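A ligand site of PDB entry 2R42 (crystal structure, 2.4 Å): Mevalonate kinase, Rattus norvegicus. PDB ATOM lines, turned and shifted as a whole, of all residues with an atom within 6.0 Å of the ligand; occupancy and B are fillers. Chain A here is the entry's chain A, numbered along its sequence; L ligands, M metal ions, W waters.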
ATOM      1  N   LYS A  13     -15.419   3.236   5.448  1.00  0.00           N
ATOM      2  CA  LYS A  13     -16.251   3.422   4.269  1.00  0.00           C
ATOM      3  C   LYS A  13     -16.216   2.232   3.314  1.00  0.00           C
ATOM      4  O   LYS A  13     -15.277   1.443   3.343  1.00  0.00           O
ATOM      5  CB  LYS A  13     -15.812   4.721   3.545  1.00  0.00           C
ATOM      6  CG  LYS A  13     -15.665   4.659   2.031  1.00  0.00           C
ATOM      7  CD  LYS A  13     -14.218   4.498   1.673  1.00  0.00           C
ATOM      8  CE  LYS A  13     -13.953   4.727   0.189  1.00  0.00           C
ATOM      9  NZ  LYS A  13     -12.485   4.625  -0.144  1.00  0.00           N
ATOM     10  N   THR A  37     -12.940   3.470  14.397  1.00  0.00           N
ATOM     11  CA  THR A  37     -11.584   3.759  14.845  1.00  0.00           C
ATOM     12  C   THR A  37     -11.791   4.581  16.118  1.00  0.00           C
ATOM     13  O   THR A  37     -12.557   5.543  16.121  1.00  0.00           O
ATOM     14  CB  THR A  37     -10.808   4.616  13.838  1.00  0.00           C
ATOM     15  OG1 THR A  37     -10.462   3.804  12.724  1.00  0.00           O
ATOM     16  CG2 THR A  37      -9.542   5.177  14.450  1.00  0.00           C
ATOM     17  N   ASN A  52       0.203   6.840  20.476  1.00  0.00           N
ATOM     18  CA  ASN A  52       0.323   5.390  20.551  1.00  0.00           C
ATOM     19  C   ASN A  52      -0.617   4.654  19.600  1.00  0.00           C
ATOM     20  O   ASN A  52      -1.832   4.817  19.635  1.00  0.00           O
ATOM     21  CB  ASN A  52       0.100   4.925  21.992  1.00  0.00           C
ATOM     22  CG  ASN A  52       0.370   3.441  22.188  1.00  0.00           C
ATOM     23  OD1 ASN A  52       1.411   2.932  21.777  1.00  0.00           O
ATOM     24  ND2 ASN A  52      -0.569   2.747  22.821  1.00  0.00           N
ATOM     25  N   LEU A  53      -0.038   3.818  18.735  1.00  0.00           N
ATOM     26  CA  LEU A  53      -0.799   3.044  17.770  1.00  0.00           C
ATOM     27  C   LEU A  53      -0.561   1.552  18.008  1.00  0.00           C
ATOM     28  O   LEU A  53       0.233   0.926  17.308  1.00  0.00           O
ATOM     29  CB  LEU A  53      -0.384   3.437  16.353  1.00  0.00           C
ATOM     30  CG  LEU A  53      -0.442   4.936  16.073  1.00  0.00           C
ATOM     31  CD1 LEU A  53       0.157   5.259  14.704  1.00  0.00           C
ATOM     32  CD2 LEU A  53      -1.897   5.386  16.156  1.00  0.00           C
ATOM     33  N   PRO A  54      -1.254   0.966  18.995  1.00  0.00           N
ATOM     34  CA  PRO A  54      -1.149  -0.445  19.368  1.00  0.00           C
ATOM     35  C   PRO A  54      -1.030  -1.386  18.165  1.00  0.00           C
ATOM     36  O   PRO A  54      -0.123  -2.230  18.123  1.00  0.00           O
ATOM     37  CB  PRO A  54      -2.430  -0.684  20.152  1.00  0.00           C
ATOM     38  CG  PRO A  54      -2.591   0.597  20.871  1.00  0.00           C
ATOM     39  CD  PRO A  54      -2.289   1.635  19.807  1.00  0.00           C
ATOM     40  N   ASN A  55      -1.930  -1.227  17.210  1.00  0.00           N
ATOM     41  CA  ASN A  55      -1.932  -2.071  16.026  1.00  0.00           C
ATOM     42  C   ASN A  55      -0.527  -2.082  15.424  1.00  0.00           C
ATOM     43  O   ASN A  55       0.215  -3.059  15.584  1.00  0.00           O
ATOM     44  CB  ASN A  55      -2.946  -1.574  15.003  1.00  0.00           C
ATOM     45  CG  ASN A  55      -4.350  -1.445  15.576  1.00  0.00           C
ATOM     46  OD1 ASN A  55      -4.680  -0.440  16.218  1.00  0.00           O
ATOM     47  ND2 ASN A  55      -5.180  -2.453  15.357  1.00  0.00           N
ATOM     48  N   VAL A  56      -0.159  -0.993  14.752  1.00  0.00           N
ATOM     49  CA  VAL A  56       1.169  -0.889  14.138  1.00  0.00           C
ATOM     50  C   VAL A  56       2.254  -0.845  15.224  1.00  0.00           C
ATOM     51  O   VAL A  56       3.368  -0.355  14.992  1.00  0.00           O
ATOM     52  CB  VAL A  56       1.271   0.370  13.250  1.00  0.00           C
ATOM     53  CG1 VAL A  56       2.586   0.358  12.480  1.00  0.00           C
ATOM     54  CG2 VAL A  56       0.086   0.419  12.303  1.00  0.00           C
ATOM     55  N   GLU A 105       3.458   3.599   8.370  1.00  0.00           N
ATOM     56  CA  GLU A 105       2.586   4.423   9.208  1.00  0.00           C
ATOM     57  C   GLU A 105       3.389   5.655   9.678  1.00  0.00           C
ATOM     58  O   GLU A 105       2.982   6.409  10.579  1.00  0.00           O
ATOM     59  CB  GLU A 105       2.089   3.605  10.407  1.00  0.00           C
ATOM     60  N   SER A 108       1.677   8.809   9.255  1.00  0.00           N
ATOM     61  CA  SER A 108       0.573   8.914  10.200  1.00  0.00           C
ATOM     62  C   SER A 108       1.000   9.862  11.354  1.00  0.00           C
ATOM     63  O   SER A 108       0.233  10.747  11.736  1.00  0.00           O
ATOM     64  CB  SER A 108       0.189   7.484  10.711  1.00  0.00           C
ATOM     65  OG  SER A 108      -0.350   6.663   9.658  1.00  0.00           O
ATOM     66  N   VAL A 133      -4.791   5.292  19.794  1.00  0.00           N
ATOM     67  CA  VAL A 133      -5.660   4.945  18.666  1.00  0.00           C
ATOM     68  C   VAL A 133      -5.719   3.442  18.403  1.00  0.00           C
ATOM     69  O   VAL A 133      -4.706   2.762  18.334  1.00  0.00           O
ATOM     70  CB  VAL A 133      -5.193   5.642  17.371  1.00  0.00           C
ATOM     71  CG1 VAL A 133      -6.191   5.363  16.261  1.00  0.00           C
ATOM     72  CG2 VAL A 133      -5.072   7.129  17.600  1.00  0.00           C
ATOM     73  N   TRP A 134      -6.939   2.947  18.295  1.00  0.00           N
ATOM     74  CA  TRP A 134      -7.184   1.528  18.043  1.00  0.00           C
ATOM     75  C   TRP A 134      -8.468   1.402  17.199  1.00  0.00           C
ATOM     76  O   TRP A 134      -9.504   1.933  17.564  1.00  0.00           O
ATOM     77  CB  TRP A 134      -7.392   0.779  19.359  1.00  0.00           C
ATOM     78  CG  TRP A 134      -7.543  -0.702  19.155  1.00  0.00           C
ATOM     79  CD1 TRP A 134      -6.538  -1.610  18.964  1.00  0.00           C
ATOM     80  CD2 TRP A 134      -8.769  -1.430  19.070  1.00  0.00           C
ATOM     81  NE1 TRP A 134      -7.071  -2.861  18.753  1.00  0.00           N
ATOM     82  CE2 TRP A 134      -8.438  -2.777  18.817  1.00  0.00           C
ATOM     83  CE3 TRP A 134     -10.115  -1.074  19.181  1.00  0.00           C
ATOM     84  CZ2 TRP A 134      -9.398  -3.782  18.665  1.00  0.00           C
ATOM     85  CZ3 TRP A 134     -11.082  -2.078  19.036  1.00  0.00           C
ATOM     86  CH2 TRP A 134     -10.721  -3.404  18.781  1.00  0.00           C
ATOM     87  N   SER A 135      -8.377   0.708  16.068  1.00  0.00           N
ATOM     88  CA  SER A 135      -9.560   0.535  15.214  1.00  0.00           C
ATOM     89  C   SER A 135      -9.935  -0.901  14.924  1.00  0.00           C
ATOM     90  O   SER A 135      -9.091  -1.797  14.948  1.00  0.00           O
ATOM     91  CB  SER A 135      -9.349   1.269  13.875  1.00  0.00           C
ATOM     92  OG  SER A 135      -8.201   0.800  13.204  1.00  0.00           O
ATOM     93  N   LEU A 137     -11.117  -1.539  12.210  1.00  0.00           N
ATOM     94  CA  LEU A 137     -10.945  -1.544  10.772  1.00  0.00           C
ATOM     95  C   LEU A 137      -9.710  -2.269  10.349  1.00  0.00           C
ATOM     96  O   LEU A 137      -8.643  -2.079  10.922  1.00  0.00           O
ATOM     97  CB  LEU A 137     -10.876  -0.127  10.225  1.00  0.00           C
ATOM     98  CG  LEU A 137     -12.159   0.586   9.846  1.00  0.00           C
ATOM     99  CD1 LEU A 137     -11.852   2.049   9.597  1.00  0.00           C
ATOM    100  CD2 LEU A 137     -12.781  -0.054   8.616  1.00  0.00           C
ATOM    101  N   PRO A 138      -9.842  -3.144   9.335  1.00  0.00           N
ATOM    102  CA  PRO A 138      -8.715  -3.897   8.807  1.00  0.00           C
ATOM    103  C   PRO A 138      -7.906  -2.916   7.978  1.00  0.00           C
ATOM    104  O   PRO A 138      -8.451  -2.159   7.184  1.00  0.00           O
ATOM    105  CB  PRO A 138      -9.394  -4.944   7.932  1.00  0.00           C
ATOM    106  CG  PRO A 138     -10.707  -5.141   8.604  1.00  0.00           C
ATOM    107  CD  PRO A 138     -11.119  -3.732   8.918  1.00  0.00           C
ATOM    108  N   PRO A 139      -6.587  -2.880   8.184  1.00  0.00           N
ATOM    109  CA  PRO A 139      -5.844  -1.920   7.375  1.00  0.00           C
ATOM    110  C   PRO A 139      -5.568  -2.440   5.962  1.00  0.00           C
ATOM    111  O   PRO A 139      -5.491  -3.642   5.717  1.00  0.00           O
ATOM    112  CB  PRO A 139      -4.566  -1.726   8.194  1.00  0.00           C
ATOM    113  CG  PRO A 139      -4.356  -3.099   8.806  1.00  0.00           C
ATOM    114  CD  PRO A 139      -5.753  -3.486   9.243  1.00  0.00           C
ATOM    115  N   GLY A 140      -5.445  -1.499   5.028  1.00  0.00           N
ATOM    116  CA  GLY A 140      -5.155  -1.857   3.634  1.00  0.00           C
ATOM    117  C   GLY A 140      -6.232  -2.503   2.795  1.00  0.00           C
ATOM    118  O   GLY A 140      -5.970  -2.876   1.639  1.00  0.00           O
ATOM    119  N   ALA A 141      -7.445  -2.641   3.318  1.00  0.00           N
ATOM    120  CA  ALA A 141      -8.514  -3.277   2.549  1.00  0.00           C
ATOM    121  C   ALA A 141      -9.379  -2.236   1.821  1.00  0.00           C
ATOM    122  O   ALA A 141     -10.443  -2.560   1.287  1.00  0.00           O
ATOM    123  CB  ALA A 141      -9.386  -4.128   3.459  1.00  0.00           C
ATOM    124  N   GLY A 142      -8.902  -0.992   1.799  1.00  0.00           N
ATOM    125  CA  GLY A 142      -9.626   0.084   1.132  1.00  0.00           C
ATOM    126  C   GLY A 142     -10.891   0.531   1.845  1.00  0.00           C
ATOM    127  O   GLY A 142     -11.795   1.110   1.242  1.00  0.00           O
ATOM    128  N   LEU A 143     -10.960   0.250   3.151  1.00  0.00           N
ATOM    129  CA  LEU A 143     -12.123   0.638   3.953  1.00  0.00           C
ATOM    130  C   LEU A 143     -11.957   2.037   4.539  1.00  0.00           C
ATOM    131  O   LEU A 143     -12.667   2.414   5.482  1.00  0.00           O
ATOM    132  CB  LEU A 143     -12.342  -0.401   5.051  1.00  0.00           C
ATOM    133  CG  LEU A 143     -13.109  -1.705   4.720  1.00  0.00           C
ATOM    134  CD1 LEU A 143     -13.210  -1.929   3.209  1.00  0.00           C
ATOM    135  CD2 LEU A 143     -12.426  -2.888   5.412  1.00  0.00           C
ATOM    136  N   GLY A 144     -11.014   2.807   3.985  1.00  0.00           N
ATOM    137  CA  GLY A 144     -10.756   4.165   4.424  1.00  0.00           C
ATOM    138  C   GLY A 144     -10.246   4.405   5.832  1.00  0.00           C
ATOM    139  O   GLY A 144     -10.463   5.486   6.400  1.00  0.00           O
ATOM    140  N   SER A 145      -9.523   3.443   6.388  1.00  0.00           N
ATOM    141  CA  SER A 145      -9.030   3.549   7.750  1.00  0.00           C
ATOM    142  C   SER A 145      -8.229   4.793   8.105  1.00  0.00           C
ATOM    143  O   SER A 145      -8.337   5.288   9.238  1.00  0.00           O
ATOM    144  CB  SER A 145      -8.216   2.307   8.112  1.00  0.00           C
ATOM    145  OG  SER A 145      -7.081   2.197   7.298  1.00  0.00           O
ATOM    146  N   SER A 146      -7.441   5.338   7.180  1.00  0.00           N
ATOM    147  CA  SER A 146      -6.656   6.522   7.486  1.00  0.00           C
ATOM    148  C   SER A 146      -7.486   7.799   7.533  1.00  0.00           C
ATOM    149  O   SER A 146      -7.071   8.806   8.094  1.00  0.00           O
ATOM    150  CB  SER A 146      -5.500   6.690   6.482  1.00  0.00           C
ATOM    151  OG  SER A 146      -5.892   7.498   5.385  1.00  0.00           O
ATOM    152  N   ALA A 147      -8.665   7.762   6.929  1.00  0.00           N
ATOM    153  CA  ALA A 147      -9.538   8.926   6.955  1.00  0.00           C
ATOM    154  C   ALA A 147     -10.164   8.910   8.336  1.00  0.00           C
ATOM    155  O   ALA A 147     -10.160   9.915   9.042  1.00  0.00           O
ATOM    156  CB  ALA A 147     -10.612   8.820   5.883  1.00  0.00           C
ATOM    157  N   TYR A 149      -9.047   7.643  10.872  1.00  0.00           N
ATOM    158  CA  TYR A 149      -7.981   7.983  11.795  1.00  0.00           C
ATOM    159  C   TYR A 149      -7.768   9.504  11.857  1.00  0.00           C
ATOM    160  O   TYR A 149      -7.644  10.079  12.943  1.00  0.00           O
ATOM    161  CB  TYR A 149      -6.688   7.287  11.369  1.00  0.00           C
ATOM    162  CG  TYR A 149      -5.410   7.914  11.886  1.00  0.00           C
ATOM    163  CD1 TYR A 149      -4.708   8.847  11.131  1.00  0.00           C
ATOM    164  CD2 TYR A 149      -4.909   7.555  13.131  1.00  0.00           C
ATOM    165  CE1 TYR A 149      -3.521   9.397  11.592  1.00  0.00           C
ATOM    166  CE2 TYR A 149      -3.721   8.105  13.609  1.00  0.00           C
ATOM    167  CZ  TYR A 149      -3.023   9.025  12.837  1.00  0.00           C
ATOM    168  OH  TYR A 149      -1.838   9.531  13.307  1.00  0.00           O
ATOM    169  N   ILE A 196      -0.871  12.359   4.123  1.00  0.00           N
ATOM    170  CA  ILE A 196      -0.707  10.927   3.993  1.00  0.00           C
ATOM    171  C   ILE A 196      -1.030  10.391   2.586  1.00  0.00           C
ATOM    172  O   ILE A 196      -0.426   9.419   2.130  1.00  0.00           O
ATOM    173  CB  ILE A 196      -1.565  10.178   5.017  1.00  0.00           C
ATOM    174  CG1 ILE A 196      -1.508   8.676   4.735  1.00  0.00           C
ATOM    175  CG2 ILE A 196      -2.983  10.681   4.973  1.00  0.00           C
ATOM    176  CD1 ILE A 196      -0.194   7.991   5.142  1.00  0.00           C
ATOM    177  N   HIS A 197      -1.968  11.025   1.912  1.00  0.00           N
ATOM    178  CA  HIS A 197      -2.340  10.573   0.583  1.00  0.00           C
ATOM    179  C   HIS A 197      -2.019  11.592  -0.501  1.00  0.00           C
ATOM    180  O   HIS A 197      -2.137  11.310  -1.689  1.00  0.00           O
ATOM    181  CB  HIS A 197      -3.828  10.181   0.539  1.00  0.00           C
ATOM    182  CG  HIS A 197      -4.124   8.890   1.224  1.00  0.00           C
ATOM    183  ND1 HIS A 197      -4.103   8.745   2.600  1.00  0.00           N
ATOM    184  CD2 HIS A 197      -4.429   7.663   0.726  1.00  0.00           C
ATOM    185  CE1 HIS A 197      -4.372   7.496   2.915  1.00  0.00           C
ATOM    186  NE2 HIS A 197      -4.572   6.817   1.800  1.00  0.00           N
ATOM    187  N   ASP A 204     -13.475   9.758   1.609  1.00  0.00           N
ATOM    188  CA  ASP A 204     -13.169   8.990   2.812  1.00  0.00           C
ATOM    189  C   ASP A 204     -13.388   9.778   4.096  1.00  0.00           C
ATOM    190  O   ASP A 204     -14.121   9.339   4.964  1.00  0.00           O
ATOM    191  CB  ASP A 204     -11.731   8.507   2.781  1.00  0.00           C
ATOM    192  CG  ASP A 204     -11.493   7.504   1.671  1.00  0.00           C
ATOM    193  OD1 ASP A 204     -10.389   6.923   1.634  1.00  0.00           O
ATOM    194  OD2 ASP A 204     -12.412   7.313   0.850  1.00  0.00           O
HETATM  195  C1  LIG L   1      -4.564   2.008   2.982  1.00  0.00           C
HETATM  196  S1  LIG L   1      -5.912   1.255   3.495  1.00  0.00           S
HETATM  197  C2  LIG L   1      -3.835   2.668   4.112  1.00  0.00           C
HETATM  198  C3  LIG L   1      -3.251   2.159   5.292  1.00  0.00           C
HETATM  199  C4  LIG L   1      -2.831   0.675   5.414  1.00  0.00           C
HETATM  200  C5  LIG L   1      -3.006   3.109   6.482  1.00  0.00           C
HETATM  201  C6  LIG L   1      -4.287   3.389   7.251  1.00  0.00           C
HETATM  202  C7  LIG L   1      -4.125   3.173   8.811  1.00  0.00           C
HETATM  203  C8  LIG L   1      -4.037   4.295   9.771  1.00  0.00           C
HETATM  204  C9  LIG L   1      -4.928   4.277  11.014  1.00  0.00           C
HETATM  205  C10 LIG L   1      -3.057   5.462   9.513  1.00  0.00           C
HETATM  206  C11 LIG L   1      -4.151   4.137  12.367  1.00  0.00           C
HETATM  207  C12 LIG L   1      -4.893   3.171  13.303  1.00  0.00           C
HETATM  208  C13 LIG L   1      -4.276   1.928  13.684  1.00  0.00           C
HETATM  209  C14 LIG L   1      -3.262   1.900  14.864  1.00  0.00           C
HETATM  210  C15 LIG L   1      -4.629   0.605  12.906  1.00  0.00           C
HETATM  211  P1  LIG L   1      -7.269   2.339   3.540  1.00  0.00           P
HETATM  212  O1  LIG L   1      -8.204   1.899   4.625  1.00  0.00           O
HETATM  213  O2  LIG L   1      -6.877   3.893   3.834  1.00  0.00           O
HETATM  214  O3  LIG L   1      -7.944   2.287   2.124  1.00  0.00           O
HETATM  215 MG    MG M   1      -8.332   6.566   3.606  1.00  0.00          MG
HETATM  216  O   HOH W   1      -3.193   3.363   0.632  1.00  0.00           O
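An oxygen (O1) of the ligand sits at hydrogen-bond distance from the side-chain hydroxyl (OG) of Ser 145 (2.9 Å).
N of Gly 140 lies close to S1 of the ligand.
An oxygen (O1) of the ligand lies within hydrogen-bond range of the backbone NH (N) of Ser 145.
The backbone NH of Gly 144 lies within hydrogen-bond range of an oxygen (O1) of the ligand (3.0 Å).
N of Gly 142 lies close to O3 of the ligand (3.4 Å).
N of Val 133 is in hydrogen-bond range of O of Asn 52 (3.0 Å).
The side-chain hydroxyl (OG) of Ser 108 sits close to the backbone carbonyl oxygen (O) of Glu 105 (3.5 Å).
The backbone carbonyl oxygen (O) of Leu 143 lies within hydrogen-bond range of the backbone NH (N) of Lys 13 (2.9 Å).
The side-chain hydroxyl (OH) of Tyr 149 sits at hydrogen-bond distance from the backbone carbonyl oxygen (O) of Ser 108 (2.9 Å).
Residues that only touch the ligand: Ser 108 (3.0 Å), Asn 55 (3.1 Å), Tyr 149 (3.5 Å), Leu 143 (3.5 Å), Leu 53 (3.6 Å), Ser 135 (3.6 Å), Ser 146 (3.6 Å) and Val 133 (3.9 Å).
Hydrophobic or aromatic side chains that line the ligand: Leu 53, Val 133 and Tyr 149.
Of the 27 residues printed, 12 come within 4 Å of the ligand.
The nearest printed residue that does not touch the ligand is Pro 139 (4.1 Å).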
